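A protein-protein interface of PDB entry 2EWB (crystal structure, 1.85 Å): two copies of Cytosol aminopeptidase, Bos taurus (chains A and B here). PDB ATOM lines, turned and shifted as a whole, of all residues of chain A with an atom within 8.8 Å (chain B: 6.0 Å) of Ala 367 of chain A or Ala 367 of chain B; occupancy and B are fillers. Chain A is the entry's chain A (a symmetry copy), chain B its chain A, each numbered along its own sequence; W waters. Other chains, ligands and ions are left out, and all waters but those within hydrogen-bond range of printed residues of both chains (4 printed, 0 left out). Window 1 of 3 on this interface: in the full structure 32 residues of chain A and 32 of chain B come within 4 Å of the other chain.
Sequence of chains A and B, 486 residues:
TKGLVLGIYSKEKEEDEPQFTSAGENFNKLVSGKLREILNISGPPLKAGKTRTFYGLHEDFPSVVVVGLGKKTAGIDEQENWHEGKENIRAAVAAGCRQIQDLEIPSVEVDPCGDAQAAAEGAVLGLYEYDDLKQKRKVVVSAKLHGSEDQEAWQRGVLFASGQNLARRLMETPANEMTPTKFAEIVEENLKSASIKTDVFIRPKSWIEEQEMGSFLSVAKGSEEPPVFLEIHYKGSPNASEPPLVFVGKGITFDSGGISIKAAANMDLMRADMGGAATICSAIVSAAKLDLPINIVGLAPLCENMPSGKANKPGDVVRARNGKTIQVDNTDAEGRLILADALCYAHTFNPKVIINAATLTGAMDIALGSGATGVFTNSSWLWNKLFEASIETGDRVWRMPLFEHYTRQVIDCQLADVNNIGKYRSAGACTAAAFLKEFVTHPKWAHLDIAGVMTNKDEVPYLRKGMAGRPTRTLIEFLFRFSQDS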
ATOM      1  N   THR A 361       8.671  22.245 -20.741  1.00  0.00           N
ATOM      2  CA  THR A 361       7.240  22.499 -20.609  1.00  0.00           C
ATOM      3  C   THR A 361       6.384  22.117 -21.796  1.00  0.00           C
ATOM      4  O   THR A 361       6.802  22.231 -22.946  1.00  0.00           O
ATOM      5  CB  THR A 361       6.967  23.991 -20.321  1.00  0.00           C
ATOM      6  OG1 THR A 361       7.354  24.775 -21.458  1.00  0.00           O
ATOM      7  CG2 THR A 361       7.759  24.459 -19.106  1.00  0.00           C
ATOM      8  N   GLY A 362       5.171  21.663 -21.501  1.00  0.00           N
ATOM      9  CA  GLY A 362       4.248  21.323 -22.563  1.00  0.00           C
ATOM     10  C   GLY A 362       3.837  22.654 -23.164  1.00  0.00           C
ATOM     11  O   GLY A 362       3.443  22.737 -24.327  1.00  0.00           O
ATOM     12  N   ALA A 363       3.944  23.708 -22.360  1.00  0.00           N
ATOM     13  CA  ALA A 363       3.585  25.045 -22.815  1.00  0.00           C
ATOM     14  C   ALA A 363       4.451  25.448 -24.003  1.00  0.00           C
ATOM     15  O   ALA A 363       3.989  26.130 -24.912  1.00  0.00           O
ATOM     16  CB  ALA A 363       3.751  26.048 -21.682  1.00  0.00           C
ATOM     17  N   MET A 364       5.710  25.022 -23.995  1.00  0.00           N
ATOM     18  CA  MET A 364       6.613  25.350 -25.095  1.00  0.00           C
ATOM     19  C   MET A 364       6.109  24.682 -26.369  1.00  0.00           C
ATOM     20  O   MET A 364       6.166  25.263 -27.459  1.00  0.00           O
ATOM     21  CB  MET A 364       8.032  24.871 -24.783  1.00  0.00           C
ATOM     22  CG  MET A 364       9.090  25.394 -25.751  1.00  0.00           C
ATOM     23  SD  MET A 364       9.241  27.201 -25.714  1.00  0.00           S
ATOM     24  CE  MET A 364       8.766  27.602 -27.356  1.00  0.00           C
ATOM     25  N   ASP A 365       5.615  23.457 -26.227  1.00  0.00           N
ATOM     26  CA  ASP A 365       5.089  22.721 -27.370  1.00  0.00           C
ATOM     27  C   ASP A 365       3.853  23.443 -27.904  1.00  0.00           C
ATOM     28  O   ASP A 365       3.681  23.602 -29.110  1.00  0.00           O
ATOM     29  CB  ASP A 365       4.701  21.302 -26.965  1.00  0.00           C
ATOM     30  CG  ASP A 365       4.160  20.508 -28.131  1.00  0.00           C
ATOM     31  OD1 ASP A 365       4.950  20.190 -29.040  1.00  0.00           O
ATOM     32  OD2 ASP A 365       2.947  20.219 -28.153  1.00  0.00           O
ATOM     33  N   ILE A 366       2.990  23.873 -26.993  1.00  0.00           N
ATOM     34  CA  ILE A 366       1.781  24.582 -27.382  1.00  0.00           C
ATOM     35  C   ILE A 366       2.150  25.920 -28.014  1.00  0.00           C
ATOM     36  O   ILE A 366       1.438  26.426 -28.880  1.00  0.00           O
ATOM     37  CB  ILE A 366       0.862  24.819 -26.162  1.00  0.00           C
ATOM     38  CG1 ILE A 366       0.369  23.474 -25.625  1.00  0.00           C
ATOM     39  CG2 ILE A 366      -0.312  25.710 -26.550  1.00  0.00           C
ATOM     40  CD1 ILE A 366      -0.492  23.580 -24.386  1.00  0.00           C
ATOM     41  N   ALA A 367       3.273  26.483 -27.579  1.00  0.00           N
ATOM     42  CA  ALA A 367       3.745  27.763 -28.101  1.00  0.00           C
ATOM     43  C   ALA A 367       4.331  27.700 -29.510  1.00  0.00           C
ATOM     44  O   ALA A 367       3.880  28.414 -30.403  1.00  0.00           O
ATOM     45  CB  ALA A 367       4.779  28.363 -27.139  1.00  0.00           C
ATOM     46  N   LEU A 368       5.334  26.852 -29.711  1.00  0.00           N
ATOM     47  CA  LEU A 368       5.985  26.758 -31.018  1.00  0.00           C
ATOM     48  C   LEU A 368       6.036  25.354 -31.613  1.00  0.00           C
ATOM     49  O   LEU A 368       6.517  25.173 -32.732  1.00  0.00           O
ATOM     50  CB  LEU A 368       7.416  27.300 -30.925  1.00  0.00           C
ATOM     51  CG  LEU A 368       7.603  28.727 -30.403  1.00  0.00           C
ATOM     52  CD1 LEU A 368       9.090  29.043 -30.299  1.00  0.00           C
ATOM     53  CD2 LEU A 368       6.914  29.706 -31.333  1.00  0.00           C
ATOM     54  N   GLY A 369       5.549  24.363 -30.876  1.00  0.00           N
ATOM     55  CA  GLY A 369       5.577  23.008 -31.398  1.00  0.00           C
ATOM     56  C   GLY A 369       6.995  22.599 -31.760  1.00  0.00           C
ATOM     57  O   GLY A 369       7.939  22.933 -31.049  1.00  0.00           O
ATOM     58  N   SER A 370       7.149  21.891 -32.874  1.00  0.00           N
ATOM     59  CA  SER A 370       8.464  21.436 -33.306  1.00  0.00           C
ATOM     60  C   SER A 370       9.091  22.388 -34.320  1.00  0.00           C
ATOM     61  O   SER A 370      10.113  22.071 -34.933  1.00  0.00           O
ATOM     62  CB  SER A 370       8.360  20.035 -33.914  1.00  0.00           C
ATOM     63  OG  SER A 370       7.448  20.023 -34.994  1.00  0.00           O
ATOM     64  N   GLY A 371       8.480  23.555 -34.490  1.00  0.00           N
ATOM     65  CA  GLY A 371       9.006  24.519 -35.436  1.00  0.00           C
ATOM     66  C   GLY A 371      10.364  25.034 -35.009  1.00  0.00           C
ATOM     67  O   GLY A 371      11.257  25.216 -35.832  1.00  0.00           O
ATOM     68  N   ALA A 372      10.528  25.267 -33.711  1.00  0.00           N
ATOM     69  CA  ALA A 372      11.794  25.769 -33.208  1.00  0.00           C
ATOM     70  C   ALA A 372      11.934  25.597 -31.711  1.00  0.00           C
ATOM     71  O   ALA A 372      10.944  25.523 -30.986  1.00  0.00           O
ATOM     72  CB  ALA A 372      11.945  27.247 -33.569  1.00  0.00           C
ATOM     73  N   GLY A 374      12.642  26.892 -28.098  1.00  0.00           N
ATOM     74  CA  GLY A 374      12.452  28.182 -27.463  1.00  0.00           C
ATOM     75  C   GLY A 374      13.707  28.537 -26.694  1.00  0.00           C
ATOM     76  O   GLY A 374      14.207  27.728 -25.915  1.00  0.00           O
ATOM     77  N   PHE A 376      15.409  31.176 -24.025  1.00  0.00           N
ATOM     78  CA  PHE A 376      15.253  32.238 -23.040  1.00  0.00           C
ATOM     79  C   PHE A 376      16.665  32.631 -22.648  1.00  0.00           C
ATOM     80  O   PHE A 376      17.432  31.791 -22.183  1.00  0.00           O
ATOM     81  CB  PHE A 376      14.524  31.744 -21.789  1.00  0.00           C
ATOM     82  CG  PHE A 376      13.089  31.384 -22.019  1.00  0.00           C
ATOM     83  CD1 PHE A 376      12.740  30.132 -22.519  1.00  0.00           C
ATOM     84  CD2 PHE A 376      12.078  32.295 -21.718  1.00  0.00           C
ATOM     85  CE1 PHE A 376      11.407  29.788 -22.712  1.00  0.00           C
ATOM     86  CE2 PHE A 376      10.740  31.960 -21.907  1.00  0.00           C
ATOM     87  CZ  PHE A 376      10.404  30.702 -22.404  1.00  0.00           C
ATOM     88  N   TRP A 398      14.004  30.007 -31.493  1.00  0.00           N
ATOM     89  CA  TRP A 398      13.153  31.182 -31.491  1.00  0.00           C
ATOM     90  C   TRP A 398      13.233  31.742 -30.087  1.00  0.00           C
ATOM     91  O   TRP A 398      13.079  31.012 -29.113  1.00  0.00           O
ATOM     92  CB  TRP A 398      11.715  30.788 -31.842  1.00  0.00           C
ATOM     93  CG  TRP A 398      10.864  31.963 -32.154  1.00  0.00           C
ATOM     94  CD1 TRP A 398      10.079  32.666 -31.284  1.00  0.00           C
ATOM     95  CD2 TRP A 398      10.767  32.631 -33.413  1.00  0.00           C
ATOM     96  NE1 TRP A 398       9.501  33.734 -31.925  1.00  0.00           N
ATOM     97  CE2 TRP A 398       9.907  33.736 -33.234  1.00  0.00           C
ATOM     98  CE3 TRP A 398      11.326  32.404 -34.679  1.00  0.00           C
ATOM     99  CZ2 TRP A 398       9.593  34.617 -34.275  1.00  0.00           C
ATOM    100  CZ3 TRP A 398      11.012  33.281 -35.716  1.00  0.00           C
ATOM    101  CH2 TRP A 398      10.153  34.374 -35.504  1.00  0.00           C
ATOM    102  N   ARG A 399      13.485  33.039 -29.975  1.00  0.00           N
ATOM    103  CA  ARG A 399      13.616  33.629 -28.658  1.00  0.00           C
ATOM    104  C   ARG A 399      12.292  33.765 -27.928  1.00  0.00           C
ATOM    105  O   ARG A 399      11.259  34.051 -28.530  1.00  0.00           O
ATOM    106  CB  ARG A 399      14.293  34.996 -28.750  1.00  0.00           C
ATOM    107  CG  ARG A 399      14.848  35.459 -27.420  1.00  0.00           C
ATOM    108  CD  ARG A 399      15.599  36.771 -27.535  1.00  0.00           C
ATOM    109  NE  ARG A 399      16.287  37.087 -26.286  1.00  0.00           N
ATOM    110  CZ  ARG A 399      17.133  38.101 -26.137  1.00  0.00           C
ATOM    111  NH1 ARG A 399      17.392  38.900 -27.162  1.00  0.00           N
ATOM    112  NH2 ARG A 399      17.723  38.309 -24.965  1.00  0.00           N
ATOM    113  N   MET A 400      12.343  33.539 -26.621  1.00  0.00           N
ATOM    114  CA  MET A 400      11.175  33.655 -25.762  1.00  0.00           C
ATOM    115  C   MET A 400      11.594  34.621 -24.657  1.00  0.00           C
ATOM    116  O   MET A 400      12.765  34.669 -24.277  1.00  0.00           O
ATOM    117  CB  MET A 400      10.792  32.289 -25.199  1.00  0.00           C
ATOM    118  CG  MET A 400      10.302  31.311 -26.261  1.00  0.00           C
ATOM    119  SD  MET A 400       8.731  31.802 -27.014  1.00  0.00           S
ATOM    120  CE  MET A 400       7.587  31.172 -25.783  1.00  0.00           C
ATOM    121  N   PRO A 401      10.640  35.392 -24.118  1.00  0.00           N
ATOM    122  CA  PRO A 401      10.892  36.384 -23.068  1.00  0.00           C
ATOM    123  C   PRO A 401      11.265  35.996 -21.644  1.00  0.00           C
ATOM    124  O   PRO A 401      10.649  35.124 -21.031  1.00  0.00           O
ATOM    125  CB  PRO A 401       9.617  37.215 -23.088  1.00  0.00           C
ATOM    126  CG  PRO A 401       8.577  36.169 -23.327  1.00  0.00           C
ATOM    127  CD  PRO A 401       9.200  35.329 -24.437  1.00  0.00           C
ATOM    128  N   TYR A 406       7.019  37.415 -15.530  1.00  0.00           N
ATOM    129  CA  TYR A 406       6.880  35.992 -15.238  1.00  0.00           C
ATOM    130  C   TYR A 406       7.503  35.628 -13.894  1.00  0.00           C
ATOM    131  O   TYR A 406       6.975  34.786 -13.170  1.00  0.00           O
ATOM    132  CB  TYR A 406       7.514  35.176 -16.363  1.00  0.00           C
ATOM    133  CG  TYR A 406       6.955  35.539 -17.722  1.00  0.00           C
ATOM    134  CD1 TYR A 406       5.625  35.267 -18.046  1.00  0.00           C
ATOM    135  CD2 TYR A 406       7.744  36.188 -18.668  1.00  0.00           C
ATOM    136  CE1 TYR A 406       5.094  35.635 -19.280  1.00  0.00           C
ATOM    137  CE2 TYR A 406       7.223  36.565 -19.906  1.00  0.00           C
ATOM    138  CZ  TYR A 406       5.899  36.284 -20.205  1.00  0.00           C
ATOM    139  OH  TYR A 406       5.379  36.655 -21.423  1.00  0.00           O
ATOM    140  N   ARG A 425      -1.878  29.711 -15.039  1.00  0.00           N
ATOM    141  CA  ARG A 425      -1.524  28.636 -15.957  1.00  0.00           C
ATOM    142  C   ARG A 425      -0.992  29.152 -17.292  1.00  0.00           C
ATOM    143  O   ARG A 425      -0.561  28.374 -18.140  1.00  0.00           O
ATOM    144  CB  ARG A 425      -2.742  27.737 -16.190  1.00  0.00           C
ATOM    145  N   SER A 426      -1.009  30.467 -17.466  1.00  0.00           N
ATOM    146  CA  SER A 426      -0.547  31.087 -18.703  1.00  0.00           C
ATOM    147  C   SER A 426       0.973  31.194 -18.801  1.00  0.00           C
ATOM    148  O   SER A 426       1.667  31.250 -17.788  1.00  0.00           O
ATOM    149  CB  SER A 426      -1.154  32.484 -18.828  1.00  0.00           C
ATOM    150  OG  SER A 426      -2.561  32.431 -18.683  1.00  0.00           O
ATOM    151  N   ALA A 427       1.475  31.224 -20.034  1.00  0.00           N
ATOM    152  CA  ALA A 427       2.905  31.357 -20.306  1.00  0.00           C
ATOM    153  C   ALA A 427       3.761  30.364 -19.530  1.00  0.00           C
ATOM    154  O   ALA A 427       4.792  30.732 -18.966  1.00  0.00           O
ATOM    155  CB  ALA A 427       3.355  32.782 -19.998  1.00  0.00           C
ATOM    156  N   GLY A 428       3.338  29.105 -19.531  1.00  0.00           N
ATOM    157  CA  GLY A 428       4.054  28.066 -18.811  1.00  0.00           C
ATOM    158  C   GLY A 428       5.547  27.974 -19.066  1.00  0.00           C
ATOM    159  O   GLY A 428       6.316  27.718 -18.141  1.00  0.00           O
ATOM    160  N   ALA A 429       5.972  28.161 -20.310  1.00  0.00           N
ATOM    161  CA  ALA A 429       7.397  28.079 -20.619  1.00  0.00           C
ATOM    162  C   ALA A 429       8.137  29.288 -20.058  1.00  0.00           C
ATOM    163  O   ALA A 429       9.294  29.184 -19.658  1.00  0.00           O
ATOM    164  CB  ALA A 429       7.610  27.989 -22.129  1.00  0.00           C
ATOM    165  N   CYS A 430       7.456  30.430 -20.022  1.00  0.00           N
ATOM    166  CA  CYS A 430       8.051  31.665 -19.522  1.00  0.00           C
ATOM    167  C   CYS A 430       8.210  31.682 -18.006  1.00  0.00           C
ATOM    168  O   CYS A 430       9.207  32.191 -17.488  1.00  0.00           O
ATOM    169  CB  CYS A 430       7.213  32.863 -19.967  1.00  0.00           C
ATOM    170  SG  CYS A 430       7.084  33.015 -21.759  1.00  0.00           S
ATOM    171  N   THR A 431       7.229  31.144 -17.289  1.00  0.00           N
ATOM    172  CA  THR A 431       7.326  31.110 -15.837  1.00  0.00           C
ATOM    173  C   THR A 431       8.336  30.040 -15.442  1.00  0.00           C
ATOM    174  O   THR A 431       9.041  30.183 -14.447  1.00  0.00           O
ATOM    175  CB  THR A 431       5.963  30.813 -15.174  1.00  0.00           C
ATOM    176  OG1 THR A 431       5.365  29.665 -15.789  1.00  0.00           O
ATOM    177  CG2 THR A 431       5.033  32.012 -15.318  1.00  0.00           C
ATOM    178  N   ASP A 449      14.205  25.474 -24.086  1.00  0.00           N
ATOM    179  CA  ASP A 449      13.107  24.575 -23.760  1.00  0.00           C
ATOM    180  C   ASP A 449      12.897  23.789 -25.044  1.00  0.00           C
ATOM    181  O   ASP A 449      12.378  24.319 -26.020  1.00  0.00           O
ATOM    182  CB  ASP A 449      11.838  25.358 -23.413  1.00  0.00           C
ATOM    183  CG  ASP A 449      10.776  24.485 -22.774  1.00  0.00           C
ATOM    184  OD1 ASP A 449      10.739  23.274 -23.083  1.00  0.00           O
ATOM    185  OD2 ASP A 449       9.974  25.007 -21.974  1.00  0.00           O
ATOM    186  N   GLY A 452       9.074  21.023 -27.230  1.00  0.00           N
ATOM    187  CA  GLY A 452       8.361  21.002 -28.495  1.00  0.00           C
ATOM    188  C   GLY A 452       9.075  20.281 -29.628  1.00  0.00           C
ATOM    189  O   GLY A 452       8.436  19.786 -30.553  1.00  0.00           O
ATOM    190  N   GLY B 362      -5.916  30.300 -27.562  1.00  0.00           N
ATOM    191  CA  GLY B 362      -5.608  30.087 -26.164  1.00  0.00           C
ATOM    192  C   GLY B 362      -4.139  29.708 -26.142  1.00  0.00           C
ATOM    193  O   GLY B 362      -3.445  29.895 -25.143  1.00  0.00           O
ATOM    194  N   ALA B 363      -3.662  29.180 -27.265  1.00  0.00           N
ATOM    195  CA  ALA B 363      -2.267  28.776 -27.377  1.00  0.00           C
ATOM    196  C   ALA B 363      -1.352  29.975 -27.163  1.00  0.00           C
ATOM    197  O   ALA B 363      -0.274  29.847 -26.590  1.00  0.00           O
ATOM    198  CB  ALA B 363      -2.007  28.155 -28.743  1.00  0.00           C
ATOM    199  N   MET B 364      -1.784  31.144 -27.623  1.00  0.00           N
ATOM    200  CA  MET B 364      -0.980  32.352 -27.457  1.00  0.00           C
ATOM    201  C   MET B 364      -0.864  32.672 -25.971  1.00  0.00           C
ATOM    202  O   MET B 364       0.195  33.095 -25.491  1.00  0.00           O
ATOM    203  CB  MET B 364      -1.624  33.529 -28.192  1.00  0.00           C
ATOM    204  CG  MET B 364      -0.731  34.762 -28.292  1.00  0.00           C
ATOM    205  SD  MET B 364       0.785  34.455 -29.240  1.00  0.00           S
ATOM    206  CE  MET B 364       2.003  34.723 -28.005  1.00  0.00           C
ATOM    207  N   ASP B 365      -1.957  32.469 -25.244  1.00  0.00           N
ATOM    208  CA  ASP B 365      -1.965  32.724 -23.809  1.00  0.00           C
ATOM    209  C   ASP B 365      -1.009  31.751 -23.123  1.00  0.00           C
ATOM    210  O   ASP B 365      -0.238  32.130 -22.244  1.00  0.00           O
ATOM    211  CB  ASP B 365      -3.366  32.533 -23.236  1.00  0.00           C
ATOM    212  CG  ASP B 365      -3.412  32.800 -21.749  1.00  0.00           C
ATOM    213  OD1 ASP B 365      -3.253  33.972 -21.360  1.00  0.00           O
ATOM    214  OD2 ASP B 365      -3.584  31.842 -20.970  1.00  0.00           O
ATOM    215  N   ILE B 366      -1.069  30.489 -23.528  1.00  0.00           N
ATOM    216  CA  ILE B 366      -0.200  29.474 -22.953  1.00  0.00           C
ATOM    217  C   ILE B 366       1.251  29.774 -23.317  1.00  0.00           C
ATOM    218  O   ILE B 366       2.168  29.453 -22.564  1.00  0.00           O
ATOM    219  CB  ILE B 366      -0.583  28.066 -23.462  1.00  0.00           C
ATOM    220  CG1 ILE B 366      -1.984  27.707 -22.962  1.00  0.00           C
ATOM    221  CG2 ILE B 366       0.439  27.039 -22.990  1.00  0.00           C
ATOM    222  CD1 ILE B 366      -2.492  26.369 -23.453  1.00  0.00           C
ATOM    223  N   ALA B 367       1.447  30.399 -24.474  1.00  0.00           N
ATOM    224  CA  ALA B 367       2.786  30.748 -24.942  1.00  0.00           C
ATOM    225  C   ALA B 367       3.433  31.920 -24.207  1.00  0.00           C
ATOM    226  O   ALA B 367       4.529  31.787 -23.667  1.00  0.00           O
ATOM    227  CB  ALA B 367       2.746  31.042 -26.447  1.00  0.00           C
ATOM    228  N   LEU B 368       2.762  33.067 -24.187  1.00  0.00           N
ATOM    229  CA  LEU B 368       3.326  34.254 -23.545  1.00  0.00           C
ATOM    230  C   LEU B 368       2.434  34.901 -22.490  1.00  0.00           C
ATOM    231  O   LEU B 368       2.835  35.876 -21.854  1.00  0.00           O
ATOM    232  CB  LEU B 368       3.666  35.307 -24.607  1.00  0.00           C
ATOM    233  CG  LEU B 368       4.604  34.892 -25.744  1.00  0.00           C
ATOM    234  CD1 LEU B 368       4.742  36.038 -26.737  1.00  0.00           C
ATOM    235  CD2 LEU B 368       5.957  34.510 -25.177  1.00  0.00           C
ATOM    236  N   GLY B 369       1.231  34.372 -22.302  1.00  0.00           N
ATOM    237  CA  GLY B 369       0.344  34.954 -21.311  1.00  0.00           C
ATOM    238  C   GLY B 369       0.109  36.428 -21.596  1.00  0.00           C
ATOM    239  O   GLY B 369      -0.024  36.824 -22.751  1.00  0.00           O
ATOM    240  N   MET B 400       6.503  36.055 -33.157  1.00  0.00           N
ATOM    241  CA  MET B 400       6.217  34.630 -33.221  1.00  0.00           C
ATOM    242  C   MET B 400       6.447  34.248 -34.680  1.00  0.00           C
ATOM    243  O   MET B 400       6.230  35.059 -35.583  1.00  0.00           O
ATOM    244  CB  MET B 400       4.779  34.358 -32.788  1.00  0.00           C
ATOM    245  CG  MET B 400       4.522  34.662 -31.317  1.00  0.00           C
ATOM    246  SD  MET B 400       5.412  33.559 -30.192  1.00  0.00           S
ATOM    247  CE  MET B 400       4.295  32.154 -30.186  1.00  0.00           C
ATOM    248  N   PRO B 401       6.875  33.003 -34.932  1.00  0.00           N
ATOM    249  CA  PRO B 401       7.164  32.498 -36.278  1.00  0.00           C
ATOM    250  C   PRO B 401       6.075  32.242 -37.310  1.00  0.00           C
ATOM    251  O   PRO B 401       5.044  31.633 -37.023  1.00  0.00           O
ATOM    252  CB  PRO B 401       7.950  31.227 -35.990  1.00  0.00           C
ATOM    253  CG  PRO B 401       7.234  30.694 -34.791  1.00  0.00           C
ATOM    254  CD  PRO B 401       7.061  31.938 -33.928  1.00  0.00           C
ATOM    255  N   TYR B 406       4.334  25.436 -40.150  1.00  0.00           N
ATOM    256  CA  TYR B 406       2.976  25.511 -39.623  1.00  0.00           C
ATOM    257  C   TYR B 406       1.936  25.500 -40.738  1.00  0.00           C
ATOM    258  O   TYR B 406       0.869  24.906 -40.591  1.00  0.00           O
ATOM    259  CB  TYR B 406       2.830  26.767 -38.764  1.00  0.00           C
ATOM    260  CG  TYR B 406       3.873  26.840 -37.671  1.00  0.00           C
ATOM    261  CD1 TYR B 406       3.878  25.919 -36.622  1.00  0.00           C
ATOM    262  CD2 TYR B 406       4.877  27.804 -37.706  1.00  0.00           C
ATOM    263  CE1 TYR B 406       4.860  25.956 -35.634  1.00  0.00           C
ATOM    264  CE2 TYR B 406       5.868  27.850 -36.724  1.00  0.00           C
ATOM    265  CZ  TYR B 406       5.852  26.924 -35.693  1.00  0.00           C
ATOM    266  OH  TYR B 406       6.827  26.963 -34.723  1.00  0.00           O
ATOM    267  N   SER B 426      -0.176  21.100 -31.357  1.00  0.00           N
ATOM    268  CA  SER B 426       0.970  21.928 -30.999  1.00  0.00           C
ATOM    269  C   SER B 426       1.034  23.247 -31.767  1.00  0.00           C
ATOM    270  O   SER B 426       0.521  23.353 -32.879  1.00  0.00           O
ATOM    271  CB  SER B 426       2.258  21.143 -31.247  1.00  0.00           C
ATOM    272  OG  SER B 426       2.211  19.887 -30.596  1.00  0.00           O
ATOM    273  N   ALA B 427       1.673  24.243 -31.159  1.00  0.00           N
ATOM    274  CA  ALA B 427       1.854  25.559 -31.768  1.00  0.00           C
ATOM    275  C   ALA B 427       0.560  26.158 -32.304  1.00  0.00           C
ATOM    276  O   ALA B 427       0.528  26.689 -33.415  1.00  0.00           O
ATOM    277  CB  ALA B 427       2.888  25.469 -32.886  1.00  0.00           C
ATOM    278  N   GLY B 428      -0.492  26.090 -31.497  1.00  0.00           N
ATOM    279  CA  GLY B 428      -1.789  26.606 -31.898  1.00  0.00           C
ATOM    280  C   GLY B 428      -1.813  28.021 -32.447  1.00  0.00           C
ATOM    281  O   GLY B 428      -2.551  28.304 -33.389  1.00  0.00           O
ATOM    282  N   ALA B 429      -1.030  28.920 -31.864  1.00  0.00           N
ATOM    283  CA  ALA B 429      -1.013  30.300 -32.343  1.00  0.00           C
ATOM    284  C   ALA B 429      -0.311  30.389 -33.693  1.00  0.00           C
ATOM    285  O   ALA B 429      -0.667  31.214 -34.531  1.00  0.00           O
ATOM    286  CB  ALA B 429      -0.318  31.207 -31.329  1.00  0.00           C
ATOM    287  N   CYS B 430       0.680  29.526 -33.899  1.00  0.00           N
ATOM    288  CA  CYS B 430       1.444  29.513 -35.142  1.00  0.00           C
ATOM    289  C   CYS B 430       0.664  28.938 -36.318  1.00  0.00           C
ATOM    290  O   CYS B 430       0.778  29.429 -37.444  1.00  0.00           O
ATOM    291  CB  CYS B 430       2.741  28.728 -34.947  1.00  0.00           C
ATOM    292  SG  CYS B 430       3.807  29.419 -33.668  1.00  0.00           S
HETATM  293  O   HOH W   1       3.208  17.042 -29.210  1.00  0.00           O
HETATM  294  O   HOH W   2      -5.760  33.295 -18.865  1.00  0.00           O
HETATM  295  O   HOH W   3       4.780  29.325 -22.603  1.00  0.00           O
HETATM  296  O   HOH W   4       1.215  28.703 -30.146  1.00  0.00           O
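The side-chain carboxylate (OD2) of Asp 365 of chain B lies within hydrogen-bond range of the side-chain hydroxyl (OG) of Ser 426 of chain A (2.6 Å). The backbone NH (N) of Ala 427 of chain A is in hydrogen-bond range of the backbone carbonyl oxygen (O) of Asp 365 of chain B (2.9 Å). The backbone NH (N) of Ala 427 of chain A sits close to the backbone carbonyl oxygen (O) of Ile 366 of chain B. O of Ile 366 of chain B lies within hydrogen-bond range of N of Gly 428 of chain A. The side-chain sulfur (SG) of Cys 430 of chain A lies within hydrogen-bond range of the backbone carbonyl oxygen (O) of Ala 367 of chain B (3.4 Å). The side-chain hydroxyl (OH) of Tyr 406 of chain A sits at hydrogen-bond distance from the backbone carbonyl oxygen (O) of Leu 368 of chain B. The side-chain hydroxyl (OH) of Tyr 406 of chain B sits at hydrogen-bond distance from the backbone carbonyl oxygen (O) of Leu 368 of chain A (2.7 Å). The side-chain carboxylate of Asp 365 of chain A is in hydrogen-bond range of the side-chain hydroxyl of Ser 426 of chain B (2.6 Å). The backbone NH (N) of Ala 427 of chain B lies close to the backbone carbonyl oxygen (O) of Ile 366 of chain A (3.2 Å). The side-chain sulfur (SG) of Cys 430 of chain B lies within hydrogen-bond range of the backbone carbonyl oxygen (O) of Ala 367 of chain A, 3.4 Å away.
O of Ala 427 of chain A is in hydrogen-bond range of OG1 of Thr 431 of chain A (3.4 Å). The side-chain hydroxyl (OG1) of Thr 431 of chain A lies within hydrogen-bond range of the backbone carbonyl oxygen (O) of Gly 428 of chain A.
CD of Pro 401 of chain A touches CD2 of Leu 368 of chain B, 3.4 Å away. Gly 369 of chain B touches Ser 426 of chain A (CA to CB, 3.8 Å). C of Leu 368 of chain B touches CB of Ala 427 of chain A (3.4 Å).
Of chain A, only Ala 367 (3.4 Å), Met 400 (3.8 Å), Ala 427 (3.8 Å) and Cys 430 (3.4 Å) come within 4 Å of Ala 367 of chain B. Of the printed residues of chain B, Tyr 406 of chain A touches Leu 368 (2.7 Å). Of the printed residues of chain B, Trp 398 of chain A touches Met 400 (3.2 Å) and Pro 401 (3.2 Å). The nearest residue of chain A that does not touch Ala 367 of chain B is Ala 363 of chain A (4.8 Å).
Of the 28 printed residues of chain A, 15 touch a printed residue of chain B. Hydrophobic or aromatic side chains of chain A that line the printed part of chain B: Ala 363, Ile 366, Ala 367, Leu 368, Trp 398, Met 400, Pro 401, Tyr 406 and Ala 427. Of the 16 printed residues of chain B, 13 touch a printed residue of chain A. Among the printed residues, 35 pairs touch across the chains. Among the printed residues, no Asp or Glu carboxylate lies within 4 Å of a Lys or Arg side-chain nitrogen of the other chain.
Of the 35 pairs that touch across the chains among the printed residues, 32 have their exchanged pair printed and touching as well.
Water W3 lies within hydrogen-bond range of the backbone carbonyl oxygen (O) of Ile 366 of chain B, the backbone carbonyl oxygen (O) of Ala 367 of chain B, the backbone NH (N) of Ala 429 of chain A and the backbone NH (N) of Gly 428 of chain A.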
